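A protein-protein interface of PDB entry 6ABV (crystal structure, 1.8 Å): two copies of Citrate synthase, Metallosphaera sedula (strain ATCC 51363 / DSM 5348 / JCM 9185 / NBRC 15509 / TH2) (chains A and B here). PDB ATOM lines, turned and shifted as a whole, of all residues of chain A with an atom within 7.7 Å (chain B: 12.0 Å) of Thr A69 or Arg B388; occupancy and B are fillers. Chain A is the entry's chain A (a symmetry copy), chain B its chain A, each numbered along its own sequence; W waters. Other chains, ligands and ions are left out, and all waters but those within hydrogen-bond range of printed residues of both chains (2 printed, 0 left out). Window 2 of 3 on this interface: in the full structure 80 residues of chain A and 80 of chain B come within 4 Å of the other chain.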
ATOM      1  N   TYR A  44     -28.227   5.604  17.019  1.00  0.00           N
ATOM      2  CA  TYR A  44     -26.936   5.643  17.626  1.00  0.00           C
ATOM      3  C   TYR A  44     -26.533   4.271  18.117  1.00  0.00           C
ATOM      4  O   TYR A  44     -27.278   3.643  18.850  1.00  0.00           O
ATOM      5  CB  TYR A  44     -26.918   6.599  18.823  1.00  0.00           C
ATOM      6  CG  TYR A  44     -27.163   8.031  18.416  1.00  0.00           C
ATOM      7  CD1 TYR A  44     -26.129   8.780  17.816  1.00  0.00           C
ATOM      8  CD2 TYR A  44     -28.391   8.679  18.624  1.00  0.00           C
ATOM      9  CE1 TYR A  44     -26.317  10.109  17.458  1.00  0.00           C
ATOM     10  CE2 TYR A  44     -28.584  10.026  18.216  1.00  0.00           C
ATOM     11  CZ  TYR A  44     -27.517  10.717  17.657  1.00  0.00           C
ATOM     12  OH  TYR A  44     -27.663  12.018  17.229  1.00  0.00           O
ATOM     13  N   LEU A  49     -23.136   5.195  22.347  1.00  0.00           N
ATOM     14  CA  LEU A  49     -23.914   5.781  23.494  1.00  0.00           C
ATOM     15  C   LEU A  49     -23.286   5.507  24.820  1.00  0.00           C
ATOM     16  O   LEU A  49     -23.156   6.396  25.677  1.00  0.00           O
ATOM     17  CB  LEU A  49     -25.365   5.351  23.422  1.00  0.00           C
ATOM     18  CG  LEU A  49     -26.238   5.774  22.253  1.00  0.00           C
ATOM     19  CD1 LEU A  49     -27.524   5.037  22.281  1.00  0.00           C
ATOM     20  CD2 LEU A  49     -26.481   7.285  22.283  1.00  0.00           C
ATOM     21  N   HIS A  52     -19.697   7.544  25.131  1.00  0.00           N
ATOM     22  CA  HIS A  52     -19.698   9.001  24.933  1.00  0.00           C
ATOM     23  C   HIS A  52     -20.946   9.701  25.455  1.00  0.00           C
ATOM     24  O   HIS A  52     -21.073  10.920  25.260  1.00  0.00           O
ATOM     25  CB  HIS A  52     -19.551   9.342  23.478  1.00  0.00           C
ATOM     26  CG  HIS A  52     -18.342   8.745  22.819  1.00  0.00           C
ATOM     27  ND1 HIS A  52     -17.051   9.078  23.175  1.00  0.00           N
ATOM     28  CD2 HIS A  52     -18.239   7.893  21.773  1.00  0.00           C
ATOM     29  CE1 HIS A  52     -16.201   8.391  22.422  1.00  0.00           C
ATOM     30  NE2 HIS A  52     -16.894   7.672  21.554  1.00  0.00           N
ATOM     31  N   THR A  53     -21.909   8.985  26.041  1.00  0.00           N
ATOM     32  CA  THR A  53     -23.086   9.715  26.574  1.00  0.00           C
ATOM     33  C   THR A  53     -23.343   9.308  28.032  1.00  0.00           C
ATOM     34  O   THR A  53     -22.433   9.255  28.796  1.00  0.00           O
ATOM     35  CB  THR A  53     -24.347   9.621  25.718  1.00  0.00           C
ATOM     36  OG1 THR A  53     -25.034   8.363  25.875  1.00  0.00           O
ATOM     37  CG2 THR A  53     -24.095   9.907  24.243  1.00  0.00           C
ATOM     38  N   SER A  54     -24.612   9.120  28.408  1.00  0.00           N
ATOM     39  CA  SER A  54     -24.979   8.954  29.806  1.00  0.00           C
ATOM     40  C   SER A  54     -26.441   8.534  29.822  1.00  0.00           C
ATOM     41  O   SER A  54     -27.120   8.620  28.824  1.00  0.00           O
ATOM     42  CB  SER A  54     -24.813  10.213  30.677  1.00  0.00           C
ATOM     43  OG  SER A  54     -25.682  11.250  30.209  1.00  0.00           O
ATOM     44  N   GLU A  57     -28.755  11.364  29.103  1.00  0.00           N
ATOM     45  CA  GLU A  57     -28.820  11.682  27.677  1.00  0.00           C
ATOM     46  C   GLU A  57     -29.621  10.694  26.870  1.00  0.00           C
ATOM     47  O   GLU A  57     -30.297  11.029  25.915  1.00  0.00           O
ATOM     48  CB  GLU A  57     -27.369  11.837  27.040  1.00  0.00           C
ATOM     49  CG  GLU A  57     -26.680  13.064  27.532  1.00  0.00           C
ATOM     50  CD  GLU A  57     -25.174  13.137  27.205  1.00  0.00           C
ATOM     51  OE1 GLU A  57     -24.846  13.763  26.205  1.00  0.00           O
ATOM     52  OE2 GLU A  57     -24.347  12.593  27.945  1.00  0.00           O
ATOM     53  N   HIS A  60     -33.289  11.320  27.324  1.00  0.00           N
ATOM     54  CA  HIS A  60     -33.716  12.371  26.433  1.00  0.00           C
ATOM     55  C   HIS A  60     -33.896  11.844  25.024  1.00  0.00           C
ATOM     56  O   HIS A  60     -34.837  12.164  24.377  1.00  0.00           O
ATOM     57  CB  HIS A  60     -32.705  13.584  26.447  1.00  0.00           C
ATOM     58  CG  HIS A  60     -33.239  14.811  25.815  1.00  0.00           C
ATOM     59  ND1 HIS A  60     -33.260  15.021  24.442  1.00  0.00           N
ATOM     60  CD2 HIS A  60     -33.792  15.917  26.373  1.00  0.00           C
ATOM     61  CE1 HIS A  60     -33.858  16.182  24.184  1.00  0.00           C
ATOM     62  NE2 HIS A  60     -34.190  16.734  25.342  1.00  0.00           N
ATOM     63  N   ASP A  66     -33.773  12.842  20.178  1.00  0.00           N
ATOM     64  CA  ASP A  66     -32.387  13.253  19.930  1.00  0.00           C
ATOM     65  C   ASP A  66     -31.634  13.386  21.163  1.00  0.00           C
ATOM     66  O   ASP A  66     -32.207  13.596  22.252  1.00  0.00           O
ATOM     67  CB  ASP A  66     -32.377  14.631  19.258  1.00  0.00           C
ATOM     68  CG  ASP A  66     -32.493  14.568  17.768  1.00  0.00           C
ATOM     69  OD1 ASP A  66     -31.431  14.338  17.072  1.00  0.00           O
ATOM     70  OD2 ASP A  66     -33.624  14.860  17.301  1.00  0.00           O
ATOM     71  N   LEU A  67     -30.305  13.306  21.070  1.00  0.00           N
ATOM     72  CA  LEU A  67     -29.475  13.635  22.190  1.00  0.00           C
ATOM     73  C   LEU A  67     -29.671  15.111  22.573  1.00  0.00           C
ATOM     74  O   LEU A  67     -29.946  15.941  21.688  1.00  0.00           O
ATOM     75  CB  LEU A  67     -27.994  13.260  21.876  1.00  0.00           C
ATOM     76  CG  LEU A  67     -27.787  11.725  21.787  1.00  0.00           C
ATOM     77  CD1 LEU A  67     -26.466  11.383  21.145  1.00  0.00           C
ATOM     78  CD2 LEU A  67     -27.894  11.031  23.147  1.00  0.00           C
ATOM     79  N   PRO A  68     -29.520  15.450  23.873  1.00  0.00           N
ATOM     80  CA  PRO A  68     -29.935  16.796  24.282  1.00  0.00           C
ATOM     81  C   PRO A  68     -28.775  17.820  24.089  1.00  0.00           C
ATOM     82  O   PRO A  68     -27.594  17.475  24.192  1.00  0.00           O
ATOM     83  CB  PRO A  68     -30.195  16.649  25.774  1.00  0.00           C
ATOM     84  CG  PRO A  68     -29.215  15.614  26.180  1.00  0.00           C
ATOM     85  CD  PRO A  68     -29.212  14.631  25.039  1.00  0.00           C
ATOM     86  N   THR A  69     -29.136  19.067  23.928  1.00  0.00           N
ATOM     87  CA  THR A  69     -28.163  20.142  24.054  1.00  0.00           C
ATOM     88  C   THR A  69     -27.818  20.293  25.499  1.00  0.00           C
ATOM     89  O   THR A  69     -28.486  19.722  26.411  1.00  0.00           O
ATOM     90  CB  THR A  69     -28.769  21.496  23.571  1.00  0.00           C
ATOM     91  OG1 THR A  69     -29.882  21.816  24.401  1.00  0.00           O
ATOM     92  CG2 THR A  69     -29.261  21.438  22.059  1.00  0.00           C
ATOM     93  N   LYS A  70     -26.831  21.138  25.774  1.00  0.00           N
ATOM     94  CA  LYS A  70     -26.543  21.504  27.177  1.00  0.00           C
ATOM     95  C   LYS A  70     -27.735  22.014  28.002  1.00  0.00           C
ATOM     96  O   LYS A  70     -27.917  21.621  29.166  1.00  0.00           O
ATOM     97  CB  LYS A  70     -25.455  22.598  27.201  1.00  0.00           C
ATOM     98  CG  LYS A  70     -24.111  22.086  26.735  1.00  0.00           C
ATOM     99  CD  LYS A  70     -23.081  22.123  27.854  1.00  0.00           C
ATOM    100  CE  LYS A  70     -21.650  22.142  27.342  1.00  0.00           C
ATOM    101  NZ  LYS A  70     -20.774  21.616  28.433  1.00  0.00           N
ATOM    102  N   LEU A  71     -28.550  22.890  27.416  1.00  0.00           N
ATOM    103  CA  LEU A  71     -29.678  23.446  28.155  1.00  0.00           C
ATOM    104  C   LEU A  71     -30.763  22.370  28.412  1.00  0.00           C
ATOM    105  O   LEU A  71     -31.281  22.262  29.531  1.00  0.00           O
ATOM    106  CB  LEU A  71     -30.286  24.605  27.432  1.00  0.00           C
ATOM    107  CG  LEU A  71     -31.589  25.201  27.955  1.00  0.00           C
ATOM    108  CD1 LEU A  71     -31.340  25.899  29.285  1.00  0.00           C
ATOM    109  CD2 LEU A  71     -32.248  26.082  26.884  1.00  0.00           C
ATOM    110  N   GLN A  72     -31.083  21.613  27.380  1.00  0.00           N
ATOM    111  CA  GLN A  72     -32.078  20.524  27.480  1.00  0.00           C
ATOM    112  C   GLN A  72     -31.619  19.505  28.552  1.00  0.00           C
ATOM    113  O   GLN A  72     -32.445  18.994  29.373  1.00  0.00           O
ATOM    114  CB  GLN A  72     -32.300  19.855  26.128  1.00  0.00           C
ATOM    115  CG  GLN A  72     -33.084  20.590  25.065  1.00  0.00           C
ATOM    116  CD  GLN A  72     -33.020  19.910  23.693  1.00  0.00           C
ATOM    117  OE1 GLN A  72     -32.050  19.247  23.334  1.00  0.00           O
ATOM    118  NE2 GLN A  72     -34.061  20.053  22.941  1.00  0.00           N
ATOM    119  N   LEU A  73     -30.333  19.179  28.591  1.00  0.00           N
ATOM    120  CA  LEU A  73     -29.821  18.280  29.620  1.00  0.00           C
ATOM    121  C   LEU A  73     -29.909  18.852  31.003  1.00  0.00           C
ATOM    122  O   LEU A  73     -30.243  18.149  31.982  1.00  0.00           O
ATOM    123  CB  LEU A  73     -28.381  17.892  29.348  1.00  0.00           C
ATOM    124  CG  LEU A  73     -27.687  16.885  30.219  1.00  0.00           C
ATOM    125  CD1 LEU A  73     -28.443  15.546  30.358  1.00  0.00           C
ATOM    126  CD2 LEU A  73     -26.274  16.651  29.714  1.00  0.00           C
ATOM    127  N   GLN A  74     -29.624  20.142  31.122  1.00  0.00           N
ATOM    128  CA  GLN A  74     -29.774  20.786  32.459  1.00  0.00           C
ATOM    129  C   GLN A  74     -31.209  20.702  32.993  1.00  0.00           C
ATOM    130  O   GLN A  74     -31.451  20.416  34.194  1.00  0.00           O
ATOM    131  CB  GLN A  74     -29.342  22.260  32.358  1.00  0.00           C
ATOM    132  CG  GLN A  74     -29.383  23.027  33.655  1.00  0.00           C
ATOM    133  CD  GLN A  74     -30.170  24.351  33.538  1.00  0.00           C
ATOM    134  OE1 GLN A  74     -31.418  24.354  33.533  1.00  0.00           O
ATOM    135  NE2 GLN A  74     -29.441  25.484  33.479  1.00  0.00           N
ATOM    136  N   ARG A  75     -32.151  20.927  32.116  1.00  0.00           N
ATOM    137  CA  ARG A  75     -33.573  20.933  32.470  1.00  0.00           C
ATOM    138  C   ARG A  75     -34.017  19.489  32.845  1.00  0.00           C
ATOM    139  O   ARG A  75     -34.698  19.303  33.828  1.00  0.00           O
ATOM    140  CB  ARG A  75     -34.419  21.435  31.318  1.00  0.00           C
ATOM    141  CG  ARG A  75     -34.438  22.965  31.215  1.00  0.00           C
ATOM    142  CD  ARG A  75     -35.184  23.335  29.958  1.00  0.00           C
ATOM    143  NE  ARG A  75     -35.164  24.781  29.669  1.00  0.00           N
ATOM    144  CZ  ARG A  75     -35.294  25.282  28.440  1.00  0.00           C
ATOM    145  NH1 ARG A  75     -35.410  24.470  27.377  1.00  0.00           N
ATOM    146  NH2 ARG A  75     -35.300  26.596  28.253  1.00  0.00           N
ATOM    147  N   ARG B 380     -26.183   7.171  12.781  1.00  0.00           N
ATOM    148  CA  ARG B 380     -25.606   8.478  13.003  1.00  0.00           C
ATOM    149  C   ARG B 380     -24.655   8.366  14.136  1.00  0.00           C
ATOM    150  O   ARG B 380     -24.747   7.429  14.959  1.00  0.00           O
ATOM    151  CB  ARG B 380     -26.659   9.543  13.264  1.00  0.00           C
ATOM    152  CG  ARG B 380     -27.853   9.103  14.148  1.00  0.00           C
ATOM    153  CD  ARG B 380     -28.842  10.254  14.255  1.00  0.00           C
ATOM    154  NE  ARG B 380     -29.956   9.981  15.190  1.00  0.00           N
ATOM    155  CZ  ARG B 380     -30.770  10.910  15.679  1.00  0.00           C
ATOM    156  NH1 ARG B 380     -31.763  10.555  16.521  1.00  0.00           N
ATOM    157  NH2 ARG B 380     -30.585  12.202  15.328  1.00  0.00           N
ATOM    158  N   ASP B 381     -23.704   9.272  14.188  1.00  0.00           N
ATOM    159  CA  ASP B 381     -22.671   9.269  15.199  1.00  0.00           C
ATOM    160  C   ASP B 381     -23.009  10.221  16.288  1.00  0.00           C
ATOM    161  O   ASP B 381     -23.547  11.322  15.979  1.00  0.00           O
ATOM    162  CB  ASP B 381     -21.286   9.671  14.589  1.00  0.00           C
ATOM    163  CG  ASP B 381     -20.756   8.630  13.589  1.00  0.00           C
ATOM    164  OD1 ASP B 381     -21.009   7.411  13.747  1.00  0.00           O
ATOM    165  OD2 ASP B 381     -20.058   9.047  12.643  1.00  0.00           O
ATOM    166  N   VAL B 382     -22.690   9.845  17.536  1.00  0.00           N
ATOM    167  CA  VAL B 382     -22.762  10.760  18.676  1.00  0.00           C
ATOM    168  C   VAL B 382     -21.828  11.996  18.427  1.00  0.00           C
ATOM    169  O   VAL B 382     -20.591  11.862  18.278  1.00  0.00           O
ATOM    170  CB  VAL B 382     -22.397  10.079  20.001  1.00  0.00           C
ATOM    171  CG1 VAL B 382     -22.205  11.088  21.140  1.00  0.00           C
ATOM    172  CG2 VAL B 382     -23.481   9.078  20.377  1.00  0.00           C
ATOM    173  N   VAL B 383     -22.464  13.165  18.456  1.00  0.00           N
ATOM    174  CA  VAL B 383     -21.798  14.475  18.395  1.00  0.00           C
ATOM    175  C   VAL B 383     -21.535  14.948  19.813  1.00  0.00           C
ATOM    176  O   VAL B 383     -22.406  14.839  20.678  1.00  0.00           O
ATOM    177  CB  VAL B 383     -22.715  15.408  17.587  1.00  0.00           C
ATOM    178  CG1 VAL B 383     -22.501  16.874  17.861  1.00  0.00           C
ATOM    179  CG2 VAL B 383     -22.582  15.059  16.105  1.00  0.00           C
ATOM    180  N   PRO B 384     -20.369  15.531  20.085  1.00  0.00           N
ATOM    181  CA  PRO B 384     -20.167  16.082  21.430  1.00  0.00           C
ATOM    182  C   PRO B 384     -21.194  17.139  21.772  1.00  0.00           C
ATOM    183  O   PRO B 384     -21.650  17.854  20.908  1.00  0.00           O
ATOM    184  CB  PRO B 384     -18.787  16.715  21.364  1.00  0.00           C
ATOM    185  CG  PRO B 384     -18.152  16.038  20.227  1.00  0.00           C
ATOM    186  CD  PRO B 384     -19.204  15.786  19.219  1.00  0.00           C
ATOM    187  N   ILE B 385     -21.528  17.255  23.039  1.00  0.00           N
ATOM    188  CA  ILE B 385     -22.667  18.056  23.419  1.00  0.00           C
ATOM    189  C   ILE B 385     -22.468  19.553  23.072  1.00  0.00           C
ATOM    190  O   ILE B 385     -23.423  20.225  22.745  1.00  0.00           O
ATOM    191  CB  ILE B 385     -23.038  17.864  24.916  1.00  0.00           C
ATOM    192  CG1 ILE B 385     -24.359  18.601  25.238  1.00  0.00           C
ATOM    193  CG2 ILE B 385     -21.972  18.323  25.882  1.00  0.00           C
ATOM    194  CD1 ILE B 385     -24.891  18.260  26.614  1.00  0.00           C
ATOM    195  N   GLU B 386     -21.212  20.015  23.073  1.00  0.00           N
ATOM    196  CA  GLU B 386     -20.833  21.391  22.651  1.00  0.00           C
ATOM    197  C   GLU B 386     -21.285  21.710  21.221  1.00  0.00           C
ATOM    198  O   GLU B 386     -21.550  22.863  20.901  1.00  0.00           O
ATOM    199  CB  GLU B 386     -19.311  21.555  22.713  1.00  0.00           C
ATOM    200  CG  GLU B 386     -18.618  21.272  24.052  1.00  0.00           C
ATOM    201  CD  GLU B 386     -18.514  19.791  24.421  1.00  0.00           C
ATOM    202  OE1 GLU B 386     -17.902  19.490  25.463  1.00  0.00           O
ATOM    203  OE2 GLU B 386     -19.066  18.929  23.700  1.00  0.00           O
ATOM    204  N   LEU B 387     -21.309  20.694  20.375  1.00  0.00           N
ATOM    205  CA  LEU B 387     -21.675  20.805  18.950  1.00  0.00           C
ATOM    206  C   LEU B 387     -23.164  20.641  18.699  1.00  0.00           C
ATOM    207  O   LEU B 387     -23.623  20.708  17.538  1.00  0.00           O
ATOM    208  CB  LEU B 387     -20.866  19.797  18.114  1.00  0.00           C
ATOM    209  CG  LEU B 387     -19.537  20.157  17.382  1.00  0.00           C
ATOM    210  CD1 LEU B 387     -18.723  21.224  18.039  1.00  0.00           C
ATOM    211  CD2 LEU B 387     -18.678  18.904  17.208  1.00  0.00           C
ATOM    212  N   ARG B 388     -23.963  20.405  19.754  1.00  0.00           N
ATOM    213  CA  ARG B 388     -25.395  20.228  19.566  1.00  0.00           C
ATOM    214  C   ARG B 388     -26.126  21.502  19.582  1.00  0.00           C
ATOM    215  O   ARG B 388     -27.233  21.509  19.095  1.00  0.00           O
ATOM    216  CB  ARG B 388     -26.005  19.285  20.675  1.00  0.00           C
ATOM    217  CG  ARG B 388     -25.437  17.889  20.572  1.00  0.00           C
ATOM    218  CD  ARG B 388     -25.964  16.934  21.650  1.00  0.00           C
ATOM    219  NE  ARG B 388     -25.042  15.784  21.795  1.00  0.00           N
ATOM    220  CZ  ARG B 388     -24.836  15.081  22.901  1.00  0.00           C
ATOM    221  NH1 ARG B 388     -25.558  15.317  24.013  1.00  0.00           N
ATOM    222  NH2 ARG B 388     -23.949  14.087  22.868  1.00  0.00           N
HETATM  223  O   HOH W   1     -25.507  13.642  18.572  1.00  0.00           O
HETATM  224  O   HOH W   2     -22.413  13.185  25.419  1.00  0.00           O
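OH of Tyr A44 sits at hydrogen-bond distance from NH2 of Arg B380, 3.5 Å away. NH2 of Arg B380 lies within salt-bridge range of OD1 of Asp A66, 2.9 Å away. The side-chain carboxylate of Glu A57 is in salt-bridge range of the guanidinium group of Arg B388. NH1 of Arg B388 is in hydrogen-bond range of O of Pro A68, at 3.0 Å.
The backbone carbonyl oxygen of Val B383 is in hydrogen-bond range of the guanidinium group of Arg B388 (2.8 Å). The backbone carbonyl oxygen (O) of Leu A49 is in hydrogen-bond range of the side-chain hydroxyl (OG1) of Thr A53, at 2.7 Å. The side-chain hydroxyl (OG) of Ser A54 lies within hydrogen-bond range of the side-chain carboxylate (OE2) of Glu A57 (3.0 Å). The backbone carbonyl oxygen (O) of Asp A66 sits at hydrogen-bond distance from a ring nitrogen (ND1) of His A60 (2.8 Å). The side-chain hydroxyl (OG1) of Thr A69 lies close to the backbone NH (N) of Leu A71 (3.5 Å). N of Thr A69 lies within hydrogen-bond range of OE1 of Gln A72, 3.0 Å away.
Asp B381 touches Tyr A44. Tyr A44 touches Val B382 (CD1 to N, 3.6 Å). Val B382 touches Leu A49 (CG2 to CD2, 3.98 Å). His A52 touches Val B382. Thr A53 touches Val B382 (CG2 to CG1, 3.8 Å). Arg B388 touches Leu A67. Thr A69 touches Ile B385. Thr A69 touches Arg B388. CD1 of Ile B385 touches N of Lys A70 (3.6 Å). CD2 of Leu A73 touches CD1 of Ile B385 (3.8 Å).
Of chain B, only Val B382 (3.8 Å) comes within 4 Å of Thr A53. Glu A57 touches one residue of chain B. Printed residues of chain B within 4 Å of Asp A66: Arg B380. Of chain B, only Ile B385 (3.6 Å) and Arg B388 (3.0 Å) come within 4 Å of Pro A68. Thr A69 touches two residues of chain B. No residue of chain B comes within 4 Å of Leu A71. No residue of chain B comes within 4 Å of Gln A72. Leu A73 touches one residue of chain B. Printed residues of chain A within 4 Å of Arg B380: Tyr A44 (3.3 Å) and Asp A66 (2.9 Å). Of the printed residues of chain A, Val B382 touches Tyr A44 (3.6 Å), Leu A49 (3.98 Å), His A52 (3.9 Å), Thr A53 (3.8 Å) and Leu A67 (3.8 Å). Arg B388 touches four residues of chain A. The nearest printed residue of chain A that does not touch Arg B380 is Leu A67 (5.5 Å).
Of the 17 printed residues of chain A, 11 touch a printed residue of chain B. Hydrophobic or aromatic side chains of chain A within 4 Å of the printed part of chain B: Tyr A44, Leu A49, His A52, Leu A67, Pro A68 and Leu A73. Hydrophobic or aromatic side chains of chain B that line the printed part of chain A: Val B382 and Ile B385. Among the printed residues, 16 pairs touch across the chains. Among the printed residues, Asp or Glu carboxylates within 4 Å of a Lys or Arg side-chain nitrogen of the other chain: Glu A57 with Arg B388 (2.8 Å) and Asp A66 with Arg B380 (2.9 Å).
No position is printed for both chains.
Water W2 lies within hydrogen-bond range of the side-chain carboxylate of Glu A57, the backbone carbonyl oxygen of His A52 and the guanidinium group of Arg B388. Water W1 lies within hydrogen-bond range of the side-chain hydroxyl (OH) of Tyr A44 (3.0 Å) and the backbone NH (N) of Val B383 (3.1 Å).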
